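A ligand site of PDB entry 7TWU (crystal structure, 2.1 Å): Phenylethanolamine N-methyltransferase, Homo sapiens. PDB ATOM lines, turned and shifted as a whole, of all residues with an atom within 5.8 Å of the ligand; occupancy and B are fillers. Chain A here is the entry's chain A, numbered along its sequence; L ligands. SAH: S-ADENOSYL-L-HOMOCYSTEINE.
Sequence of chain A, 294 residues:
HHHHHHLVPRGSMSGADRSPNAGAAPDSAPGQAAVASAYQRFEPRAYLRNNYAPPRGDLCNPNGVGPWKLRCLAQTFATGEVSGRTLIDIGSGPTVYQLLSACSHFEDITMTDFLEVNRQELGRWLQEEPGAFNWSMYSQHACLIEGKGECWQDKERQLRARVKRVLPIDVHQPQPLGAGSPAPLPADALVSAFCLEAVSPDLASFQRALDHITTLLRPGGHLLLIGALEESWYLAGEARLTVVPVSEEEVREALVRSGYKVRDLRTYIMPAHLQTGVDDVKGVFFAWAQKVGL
The side-chain hydroxyl (OH) of Tyr 97 is in hydrogen-bond range of the side-chain hydroxyl (OH) of Tyr 52.
The side-chain amino group of Lys 69 lies within hydrogen-bond range of the side-chain hydroxyl of Tyr 52 (3.3 Å).
ND2 of Asn 118 is in hydrogen-bond range of OD2 of Asp 113, at 3.0 Å.
OH of Tyr 97 lies within hydrogen-bond range of NZ of Lys 69 (3.3 Å).
NE2 of His 172 is in hydrogen-bond range of O of Val 199 (3.1 Å).
The side-chain carboxylate (OD1) of Asp 170 is in hydrogen-bond range of the backbone NH (N) of His 172.
OH of Tyr 234 sits at hydrogen-bond distance from OH of Tyr 39, 2.7 Å away.
The side-chain hydroxyl (OH) of Tyr 39 is in hydrogen-bond range of the backbone carbonyl oxygen (O) of Ala 198, 2.8 Å away.
A sulfur (SD) of the ligand lies close to the backbone carbonyl oxygen (O) of Phe 194 (3.7 Å).
CE1 of Tyr 39 touches C2' of the ligand (3.5 Å).
Gly 93 touches the ligand.
OG1 of Thr 95 touches CA of the ligand, at 3.4 Å.
Phe 114 touches the ligand.
Leu 115 touches the ligand (CG to O2', 3.4 Å).
His 172 touches the ligand (CD2 to N6, 3.5 Å).
Val 199 touches the ligand (CG1 to C5, 3.4 Å).
OH of Tyr 234 touches SD of the ligand (3.8 Å).
20 residues have an atom within 4 Å of the ligand: Tyr 39, Tyr 47, Tyr 52, Gly 91, Ser 92, Gly 93, Thr 95, Tyr 97, Asp 113, Phe 114, Leu 115, Asn 118, Asp 170, Val 171, His 172, Ala 193, Phe 194, Cys 195, Val 199 and Tyr 234.
OH of Tyr 52 is in hydrogen-bond range of O of the ligand, 2.6 Å away.
O of the ligand sits at hydrogen-bond distance from OH of Tyr 47.
The side-chain carboxylate (OD1) of Asp 113 lies within hydrogen-bond range of an oxygen (O3') of the ligand (2.6 Å).
The backbone carbonyl oxygen of Ala 193 is in hydrogen-bond range of a nitrogen (N) of the ligand (2.6 Å).
OXT of the ligand is in hydrogen-bond range of OH of Tyr 97 (2.7 Å).
O of Gly 91 lies within hydrogen-bond range of N of the ligand, 3.0 Å away.
The side-chain amide nitrogen of Asn 118 is in hydrogen-bond range of an oxygen (O3') of the ligand.
The backbone NH (N) of Val 171 lies within hydrogen-bond range of a nitrogen (N1) of the ligand (3.1 Å).
A nitrogen (N) of the ligand sits close to the backbone carbonyl oxygen (O) of Ser 92, 3.3 Å away.
A nitrogen (N6) of the ligand lies within hydrogen-bond range of the side-chain carboxylate (OD1) of Asp 170.
The side-chain sulfur (SG) of Cys 195 sits at hydrogen-bond distance from a nitrogen (N3) of the ligand (3.4 Å).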
ATOM      1  N   VAL A  35      26.502   1.743 -25.069  1.00  0.00           N
ATOM      2  CA  VAL A  35      25.477   1.469 -24.073  1.00  0.00           C
ATOM      3  C   VAL A  35      24.693   0.211 -24.442  1.00  0.00           C
ATOM      4  O   VAL A  35      24.274  -0.535 -23.560  1.00  0.00           O
ATOM      5  CB  VAL A  35      24.548   2.697 -23.924  1.00  0.00           C
ATOM      6  CG1 VAL A  35      23.813   2.675 -22.595  1.00  0.00           C
ATOM      7  CG2 VAL A  35      25.349   3.994 -24.081  1.00  0.00           C
ATOM      8  N   TYR A  39      23.839  -3.056 -21.685  1.00  0.00           N
ATOM      9  CA  TYR A  39      22.488  -3.430 -21.279  1.00  0.00           C
ATOM     10  C   TYR A  39      22.126  -4.850 -21.656  1.00  0.00           C
ATOM     11  O   TYR A  39      21.091  -5.353 -21.205  1.00  0.00           O
ATOM     12  CB  TYR A  39      21.475  -2.432 -21.867  1.00  0.00           C
ATOM     13  CG  TYR A  39      21.294  -1.242 -20.946  1.00  0.00           C
ATOM     14  CD1 TYR A  39      20.502  -1.335 -19.789  1.00  0.00           C
ATOM     15  CD2 TYR A  39      21.943  -0.042 -21.190  1.00  0.00           C
ATOM     16  CE1 TYR A  39      20.359  -0.265 -18.931  1.00  0.00           C
ATOM     17  CE2 TYR A  39      21.791   1.046 -20.333  1.00  0.00           C
ATOM     18  CZ  TYR A  39      21.012   0.924 -19.203  1.00  0.00           C
ATOM     19  OH  TYR A  39      20.868   1.994 -18.359  1.00  0.00           O
ATOM     20  N   PHE A  42      21.927  -6.807 -18.378  1.00  0.00           N
ATOM     21  CA  PHE A  42      21.034  -6.252 -17.356  1.00  0.00           C
ATOM     22  C   PHE A  42      20.055  -7.307 -16.833  1.00  0.00           C
ATOM     23  O   PHE A  42      19.264  -7.848 -17.603  1.00  0.00           O
ATOM     24  CB  PHE A  42      20.299  -5.064 -17.976  1.00  0.00           C
ATOM     25  CG  PHE A  42      19.313  -4.359 -17.056  1.00  0.00           C
ATOM     26  CD1 PHE A  42      18.067  -4.904 -16.795  1.00  0.00           C
ATOM     27  CD2 PHE A  42      19.616  -3.110 -16.540  1.00  0.00           C
ATOM     28  CE1 PHE A  42      17.154  -4.228 -15.972  1.00  0.00           C
ATOM     29  CE2 PHE A  42      18.726  -2.436 -15.739  1.00  0.00           C
ATOM     30  CZ  PHE A  42      17.478  -2.991 -15.455  1.00  0.00           C
ATOM     31  N   TYR A  47      18.013  -5.655 -10.617  1.00  0.00           N
ATOM     32  CA  TYR A  47      17.687  -4.236 -10.541  1.00  0.00           C
ATOM     33  C   TYR A  47      16.533  -3.965  -9.559  1.00  0.00           C
ATOM     34  O   TYR A  47      16.569  -3.006  -8.785  1.00  0.00           O
ATOM     35  CB  TYR A  47      17.339  -3.706 -11.923  1.00  0.00           C
ATOM     36  CG  TYR A  47      16.965  -2.239 -11.957  1.00  0.00           C
ATOM     37  CD1 TYR A  47      17.935  -1.239 -11.938  1.00  0.00           C
ATOM     38  CD2 TYR A  47      15.631  -1.845 -12.012  1.00  0.00           C
ATOM     39  CE1 TYR A  47      17.578   0.103 -11.970  1.00  0.00           C
ATOM     40  CE2 TYR A  47      15.272  -0.514 -12.036  1.00  0.00           C
ATOM     41  CZ  TYR A  47      16.241   0.453 -12.015  1.00  0.00           C
ATOM     42  OH  TYR A  47      15.860   1.763 -12.053  1.00  0.00           O
ATOM     43  N   TYR A  52      14.112  -1.401  -5.374  1.00  0.00           N
ATOM     44  CA  TYR A  52      12.706  -1.427  -4.984  1.00  0.00           C
ATOM     45  C   TYR A  52      12.410  -2.491  -3.932  1.00  0.00           C
ATOM     46  O   TYR A  52      11.234  -2.796  -3.692  1.00  0.00           O
ATOM     47  CB  TYR A  52      11.828  -1.610  -6.225  1.00  0.00           C
ATOM     48  CG  TYR A  52      12.074  -0.464  -7.169  1.00  0.00           C
ATOM     49  CD1 TYR A  52      11.485   0.770  -6.934  1.00  0.00           C
ATOM     50  CD2 TYR A  52      12.960  -0.577  -8.255  1.00  0.00           C
ATOM     51  CE1 TYR A  52      11.724   1.835  -7.745  1.00  0.00           C
ATOM     52  CE2 TYR A  52      13.187   0.513  -9.096  1.00  0.00           C
ATOM     53  CZ  TYR A  52      12.557   1.720  -8.824  1.00  0.00           C
ATOM     54  OH  TYR A  52      12.752   2.833  -9.604  1.00  0.00           O
ATOM     55  N   LYS A  69       9.458  10.128  -4.406  1.00  0.00           N
ATOM     56  CA  LYS A  69       9.056   9.984  -5.802  1.00  0.00           C
ATOM     57  C   LYS A  69       7.542   9.895  -5.947  1.00  0.00           C
ATOM     58  O   LYS A  69       6.935  10.599  -6.768  1.00  0.00           O
ATOM     59  CB  LYS A  69       9.722   8.749  -6.412  1.00  0.00           C
ATOM     60  CG  LYS A  69      11.208   8.899  -6.633  1.00  0.00           C
ATOM     61  CD  LYS A  69      11.719   7.754  -7.477  1.00  0.00           C
ATOM     62  CE  LYS A  69      11.750   6.467  -6.720  1.00  0.00           C
ATOM     63  NZ  LYS A  69      12.404   5.419  -7.555  1.00  0.00           N
ATOM     64  N   ILE A  90       8.378   6.228 -20.925  1.00  0.00           N
ATOM     65  CA  ILE A  90       9.618   6.088 -21.688  1.00  0.00           C
ATOM     66  C   ILE A  90      10.657   5.339 -20.840  1.00  0.00           C
ATOM     67  O   ILE A  90      11.093   5.838 -19.792  1.00  0.00           O
ATOM     68  CB  ILE A  90      10.162   7.460 -22.107  1.00  0.00           C
ATOM     69  CG1 ILE A  90       9.089   8.291 -22.805  1.00  0.00           C
ATOM     70  CG2 ILE A  90      11.448   7.336 -22.934  1.00  0.00           C
ATOM     71  CD1 ILE A  90       8.904   7.956 -24.251  1.00  0.00           C
ATOM     72  N   GLY A  91      11.093   4.174 -21.314  1.00  0.00           N
ATOM     73  CA  GLY A  91      12.066   3.377 -20.584  1.00  0.00           C
ATOM     74  C   GLY A  91      11.572   2.836 -19.255  1.00  0.00           C
ATOM     75  O   GLY A  91      12.220   3.001 -18.227  1.00  0.00           O
ATOM     76  N   SER A  92      10.426   2.141 -19.287  1.00  0.00           N
ATOM     77  CA  SER A  92       9.791   1.651 -18.069  1.00  0.00           C
ATOM     78  C   SER A  92      10.687   0.736 -17.253  1.00  0.00           C
ATOM     79  O   SER A  92      10.526   0.658 -16.023  1.00  0.00           O
ATOM     80  CB  SER A  92       8.514   0.884 -18.438  1.00  0.00           C
ATOM     81  OG  SER A  92       7.616   1.706 -19.148  1.00  0.00           O
ATOM     82  N   GLY A  93      11.607   0.020 -17.889  1.00  0.00           N
ATOM     83  CA  GLY A  93      12.251  -1.083 -17.211  1.00  0.00           C
ATOM     84  C   GLY A  93      11.214  -2.078 -16.706  1.00  0.00           C
ATOM     85  O   GLY A  93      10.155  -2.257 -17.318  1.00  0.00           O
ATOM     86  N   PRO A  94      11.489  -2.736 -15.585  1.00  0.00           N
ATOM     87  CA  PRO A  94      10.522  -3.697 -15.047  1.00  0.00           C
ATOM     88  C   PRO A  94       9.663  -3.109 -13.942  1.00  0.00           C
ATOM     89  O   PRO A  94       9.271  -3.827 -13.012  1.00  0.00           O
ATOM     90  CB  PRO A  94      11.432  -4.812 -14.523  1.00  0.00           C
ATOM     91  CG  PRO A  94      12.620  -4.030 -13.992  1.00  0.00           C
ATOM     92  CD  PRO A  94      12.741  -2.756 -14.811  1.00  0.00           C
ATOM     93  N   THR A  95       9.383  -1.798 -13.986  1.00  0.00           N
ATOM     94  CA  THR A  95       8.753  -1.117 -12.865  1.00  0.00           C
ATOM     95  C   THR A  95       7.447  -0.460 -13.291  1.00  0.00           C
ATOM     96  O   THR A  95       7.305   0.004 -14.427  1.00  0.00           O
ATOM     97  CB  THR A  95       9.666  -0.046 -12.234  1.00  0.00           C
ATOM     98  OG1 THR A  95       9.766   1.083 -13.108  1.00  0.00           O
ATOM     99  CG2 THR A  95      11.061  -0.598 -11.985  1.00  0.00           C
ATOM    100  N   TYR A  97       5.637   1.564 -10.612  1.00  0.00           N
ATOM    101  CA  TYR A  97       5.291   2.575  -9.610  1.00  0.00           C
ATOM    102  C   TYR A  97       5.128   3.955 -10.217  1.00  0.00           C
ATOM    103  O   TYR A  97       4.392   4.791  -9.681  1.00  0.00           O
ATOM    104  CB  TYR A  97       6.361   2.649  -8.496  1.00  0.00           C
ATOM    105  CG  TYR A  97       7.632   3.332  -9.007  1.00  0.00           C
ATOM    106  CD1 TYR A  97       8.576   2.611  -9.706  1.00  0.00           C
ATOM    107  CD2 TYR A  97       7.822   4.692  -8.846  1.00  0.00           C
ATOM    108  CE1 TYR A  97       9.716   3.224 -10.207  1.00  0.00           C
ATOM    109  CE2 TYR A  97       8.947   5.321  -9.341  1.00  0.00           C
ATOM    110  CZ  TYR A  97       9.893   4.581 -10.017  1.00  0.00           C
ATOM    111  OH  TYR A  97      11.020   5.188 -10.518  1.00  0.00           O
ATOM    112  N   GLN A  98       5.836   4.222 -11.322  1.00  0.00           N
ATOM    113  CA  GLN A  98       5.813   5.570 -11.884  1.00  0.00           C
ATOM    114  C   GLN A  98       4.508   5.902 -12.572  1.00  0.00           C
ATOM    115  O   GLN A  98       4.339   7.048 -13.016  1.00  0.00           O
ATOM    116  CB  GLN A  98       6.979   5.755 -12.867  1.00  0.00           C
ATOM    117  CG  GLN A  98       6.912   4.893 -14.122  1.00  0.00           C
ATOM    118  CD  GLN A  98       7.602   3.557 -13.940  1.00  0.00           C
ATOM    119  OE1 GLN A  98       7.731   3.053 -12.815  1.00  0.00           O
ATOM    120  NE2 GLN A  98       8.073   2.970 -15.047  1.00  0.00           N
ATOM    121  N   ASP A 113      10.148  -0.339 -23.224  1.00  0.00           N
ATOM    122  CA  ASP A 113      11.534  -0.521 -22.814  1.00  0.00           C
ATOM    123  C   ASP A 113      12.388  -1.081 -23.956  1.00  0.00           C
ATOM    124  O   ASP A 113      11.905  -1.777 -24.850  1.00  0.00           O
ATOM    125  CB  ASP A 113      11.685  -1.448 -21.606  1.00  0.00           C
ATOM    126  CG  ASP A 113      13.043  -1.295 -20.927  1.00  0.00           C
ATOM    127  OD1 ASP A 113      13.324  -0.217 -20.351  1.00  0.00           O
ATOM    128  OD2 ASP A 113      13.853  -2.252 -20.981  1.00  0.00           O
ATOM    129  N   PHE A 114      13.687  -0.775 -23.877  1.00  0.00           N
ATOM    130  CA  PHE A 114      14.654  -1.251 -24.860  1.00  0.00           C
ATOM    131  C   PHE A 114      14.822  -2.775 -24.782  1.00  0.00           C
ATOM    132  O   PHE A 114      14.995  -3.436 -25.808  1.00  0.00           O
ATOM    133  CB  PHE A 114      15.986  -0.546 -24.629  1.00  0.00           C
ATOM    134  CG  PHE A 114      17.056  -0.889 -25.628  1.00  0.00           C
ATOM    135  CD1 PHE A 114      17.103  -0.247 -26.852  1.00  0.00           C
ATOM    136  CD2 PHE A 114      18.027  -1.825 -25.320  1.00  0.00           C
ATOM    137  CE1 PHE A 114      18.093  -0.565 -27.776  1.00  0.00           C
ATOM    138  CE2 PHE A 114      19.031  -2.138 -26.244  1.00  0.00           C
ATOM    139  CZ  PHE A 114      19.052  -1.508 -27.468  1.00  0.00           C
ATOM    140  N   LEU A 115      14.761  -3.336 -23.570  1.00  0.00           N
ATOM    141  CA  LEU A 115      15.062  -4.733 -23.314  1.00  0.00           C
ATOM    142  C   LEU A 115      13.798  -5.577 -23.295  1.00  0.00           C
ATOM    143  O   LEU A 115      12.827  -5.243 -22.600  1.00  0.00           O
ATOM    144  CB  LEU A 115      15.820  -4.918 -22.001  1.00  0.00           C
ATOM    145  CG  LEU A 115      17.192  -4.256 -21.873  1.00  0.00           C
ATOM    146  CD1 LEU A 115      17.909  -4.716 -20.606  1.00  0.00           C
ATOM    147  CD2 LEU A 115      18.010  -4.586 -23.108  1.00  0.00           C
ATOM    148  N   ASN A 118      12.839  -7.045 -19.897  1.00  0.00           N
ATOM    149  CA  ASN A 118      12.064  -6.141 -19.067  1.00  0.00           C
ATOM    150  C   ASN A 118      10.607  -6.113 -19.496  1.00  0.00           C
ATOM    151  O   ASN A 118       9.703  -6.145 -18.642  1.00  0.00           O
ATOM    152  CB  ASN A 118      12.662  -4.731 -19.120  1.00  0.00           C
ATOM    153  CG  ASN A 118      13.758  -4.531 -18.106  1.00  0.00           C
ATOM    154  OD1 ASN A 118      13.806  -5.221 -17.090  1.00  0.00           O
ATOM    155  ND2 ASN A 118      14.646  -3.587 -18.374  1.00  0.00           N
ATOM    156  N   ILE A 169      11.454   0.339 -27.618  1.00  0.00           N
ATOM    157  CA  ILE A 169      11.767   1.755 -27.800  1.00  0.00           C
ATOM    158  C   ILE A 169      13.280   1.911 -27.787  1.00  0.00           C
ATOM    159  O   ILE A 169      14.002   1.112 -27.186  1.00  0.00           O
ATOM    160  CB  ILE A 169      11.105   2.629 -26.699  1.00  0.00           C
ATOM    161  CG1 ILE A 169      11.258   4.117 -27.014  1.00  0.00           C
ATOM    162  CG2 ILE A 169      11.700   2.308 -25.328  1.00  0.00           C
ATOM    163  CD1 ILE A 169      10.456   5.013 -26.127  1.00  0.00           C
ATOM    164  N   ASP A 170      13.775   2.945 -28.475  1.00  0.00           N
ATOM    165  CA  ASP A 170      15.188   3.289 -28.446  1.00  0.00           C
ATOM    166  C   ASP A 170      15.249   4.802 -28.572  1.00  0.00           C
ATOM    167  O   ASP A 170      15.103   5.344 -29.671  1.00  0.00           O
ATOM    168  CB  ASP A 170      15.959   2.604 -29.567  1.00  0.00           C
ATOM    169  CG  ASP A 170      17.450   2.927 -29.557  1.00  0.00           C
ATOM    170  OD1 ASP A 170      17.871   3.968 -28.992  1.00  0.00           O
ATOM    171  OD2 ASP A 170      18.226   2.138 -30.139  1.00  0.00           O
ATOM    172  N   VAL A 171      15.502   5.487 -27.446  1.00  0.00           N
ATOM    173  CA  VAL A 171      15.443   6.946 -27.435  1.00  0.00           C
ATOM    174  C   VAL A 171      16.570   7.587 -28.242  1.00  0.00           C
ATOM    175  O   VAL A 171      16.575   8.809 -28.406  1.00  0.00           O
ATOM    176  CB  VAL A 171      15.463   7.492 -25.996  1.00  0.00           C
ATOM    177  CG1 VAL A 171      14.348   6.826 -25.144  1.00  0.00           C
ATOM    178  CG2 VAL A 171      16.807   7.261 -25.364  1.00  0.00           C
ATOM    179  N   HIS A 172      17.520   6.795 -28.738  1.00  0.00           N
ATOM    180  CA  HIS A 172      18.552   7.334 -29.610  1.00  0.00           C
ATOM    181  C   HIS A 172      18.071   7.504 -31.041  1.00  0.00           C
ATOM    182  O   HIS A 172      18.585   8.357 -31.773  1.00  0.00           O
ATOM    183  CB  HIS A 172      19.795   6.436 -29.572  1.00  0.00           C
ATOM    184  CG  HIS A 172      20.424   6.350 -28.217  1.00  0.00           C
ATOM    185  ND1 HIS A 172      20.721   7.469 -27.458  1.00  0.00           N
ATOM    186  CD2 HIS A 172      20.814   5.279 -27.479  1.00  0.00           C
ATOM    187  CE1 HIS A 172      21.267   7.090 -26.318  1.00  0.00           C
ATOM    188  NE2 HIS A 172      21.335   5.769 -26.303  1.00  0.00           N
ATOM    189  N   ALA A 193      11.424   7.859 -16.159  1.00  0.00           N
ATOM    190  CA  ALA A 193      12.118   7.830 -14.877  1.00  0.00           C
ATOM    191  C   ALA A 193      13.393   7.024 -15.002  1.00  0.00           C
ATOM    192  O   ALA A 193      13.343   5.827 -15.300  1.00  0.00           O
ATOM    193  CB  ALA A 193      11.233   7.253 -13.761  1.00  0.00           C
ATOM    194  N   PHE A 194      14.525   7.693 -14.769  1.00  0.00           N
ATOM    195  CA  PHE A 194      15.833   7.046 -14.712  1.00  0.00           C
ATOM    196  C   PHE A 194      16.241   6.382 -16.027  1.00  0.00           C
ATOM    197  O   PHE A 194      16.893   5.347 -16.027  1.00  0.00           O
ATOM    198  CB  PHE A 194      15.885   6.024 -13.583  1.00  0.00           C
ATOM    199  CG  PHE A 194      15.634   6.616 -12.248  1.00  0.00           C
ATOM    200  CD1 PHE A 194      16.588   7.439 -11.651  1.00  0.00           C
ATOM    201  CD2 PHE A 194      14.423   6.410 -11.604  1.00  0.00           C
ATOM    202  CE1 PHE A 194      16.339   8.006 -10.378  1.00  0.00           C
ATOM    203  CE2 PHE A 194      14.158   6.978 -10.360  1.00  0.00           C
ATOM    204  CZ  PHE A 194      15.118   7.771  -9.754  1.00  0.00           C
ATOM    205  N   CYS A 195      15.838   6.960 -17.151  1.00  0.00           N
ATOM    206  CA  CYS A 195      16.200   6.399 -18.445  1.00  0.00           C
ATOM    207  C   CYS A 195      17.285   7.227 -19.130  1.00  0.00           C
ATOM    208  O   CYS A 195      18.415   6.761 -19.270  1.00  0.00           O
ATOM    209  CB  CYS A 195      14.968   6.298 -19.353  1.00  0.00           C
ATOM    210  SG  CYS A 195      15.309   5.477 -20.934  1.00  0.00           S
ATOM    211  N   ALA A 198      20.708   7.405 -17.902  1.00  0.00           N
ATOM    212  CA  ALA A 198      21.271   6.074 -17.763  1.00  0.00           C
ATOM    213  C   ALA A 198      21.553   5.397 -19.100  1.00  0.00           C
ATOM    214  O   ALA A 198      22.145   4.322 -19.111  1.00  0.00           O
ATOM    215  CB  ALA A 198      20.315   5.192 -16.939  1.00  0.00           C
ATOM    216  N   VAL A 199      21.110   5.980 -20.203  1.00  0.00           N
ATOM    217  CA  VAL A 199      21.333   5.398 -21.531  1.00  0.00           C
ATOM    218  C   VAL A 199      22.266   6.246 -22.374  1.00  0.00           C
ATOM    219  O   VAL A 199      22.573   5.867 -23.517  1.00  0.00           O
ATOM    220  CB  VAL A 199      19.991   5.171 -22.262  1.00  0.00           C
ATOM    221  CG1 VAL A 199      19.138   4.214 -21.453  1.00  0.00           C
ATOM    222  CG2 VAL A 199      19.249   6.483 -22.457  1.00  0.00           C
ATOM    223  N   TYR A 234      25.640   2.296 -12.086  1.00  0.00           N
ATOM    224  CA  TYR A 234      24.814   1.453 -11.229  1.00  0.00           C
ATOM    225  C   TYR A 234      24.914   0.014 -11.723  1.00  0.00           C
ATOM    226  O   TYR A 234      25.264  -0.236 -12.881  1.00  0.00           O
ATOM    227  CB  TYR A 234      23.346   1.925 -11.183  1.00  0.00           C
ATOM    228  CG  TYR A 234      22.549   1.701 -12.434  1.00  0.00           C
ATOM    229  CD1 TYR A 234      22.667   2.572 -13.517  1.00  0.00           C
ATOM    230  CD2 TYR A 234      21.675   0.640 -12.541  1.00  0.00           C
ATOM    231  CE1 TYR A 234      21.928   2.380 -14.664  1.00  0.00           C
ATOM    232  CE2 TYR A 234      20.929   0.447 -13.666  1.00  0.00           C
ATOM    233  CZ  TYR A 234      21.057   1.313 -14.728  1.00  0.00           C
ATOM    234  OH  TYR A 234      20.287   1.087 -15.845  1.00  0.00           O
HETATM  235  N   SAH L   1      12.160   3.457 -15.295  1.00  0.00           N
HETATM  236  CA  SAH L   1      12.569   2.406 -14.381  1.00  0.00           C
HETATM  237  CB  SAH L   1      13.888   1.763 -14.814  1.00  0.00           C
HETATM  238  CG  SAH L   1      15.007   2.624 -15.401  1.00  0.00           C
HETATM  239  SD  SAH L   1      16.508   1.636 -15.662  1.00  0.00           S
HETATM  240  C   SAH L   1      12.679   2.959 -12.957  1.00  0.00           C
HETATM  241  O   SAH L   1      13.303   2.342 -12.091  1.00  0.00           O
HETATM  242  OXT SAH L   1      12.115   4.021 -12.660  1.00  0.00           O
HETATM  243  C5' SAH L   1      16.813   2.355 -17.308  1.00  0.00           C
HETATM  244  C4' SAH L   1      16.054   1.640 -18.428  1.00  0.00           C
HETATM  245  O4' SAH L   1      16.423   2.149 -19.713  1.00  0.00           O
HETATM  246  C3' SAH L   1      16.336   0.148 -18.486  1.00  0.00           C
HETATM  247  O3' SAH L   1      15.111  -0.556 -18.426  1.00  0.00           O
HETATM  248  C2' SAH L   1      16.948  -0.075 -19.856  1.00  0.00           C
HETATM  249  O2' SAH L   1      16.549  -1.304 -20.410  1.00  0.00           O
HETATM  250  C1' SAH L   1      16.389   1.092 -20.644  1.00  0.00           C
HETATM  251  N9  SAH L   1      17.178   1.378 -21.848  1.00  0.00           N
HETATM  252  C8  SAH L   1      18.428   0.880 -22.113  1.00  0.00           C
HETATM  253  N7  SAH L   1      18.822   1.373 -23.312  1.00  0.00           N
HETATM  254  C5  SAH L   1      17.849   2.164 -23.823  1.00  0.00           C
HETATM  255  C6  SAH L   1      17.761   2.901 -25.012  1.00  0.00           C
HETATM  256  N6  SAH L   1      18.755   2.906 -25.892  1.00  0.00           N
HETATM  257  N1  SAH L   1      16.632   3.639 -25.265  1.00  0.00           N
HETATM  258  C2  SAH L   1      15.598   3.641 -24.336  1.00  0.00           C
HETATM  259  N3  SAH L   1      15.686   2.903 -23.160  1.00  0.00           N
HETATM  260  C4  SAH L   1      16.804   2.172 -22.901  1.00  0.00           C
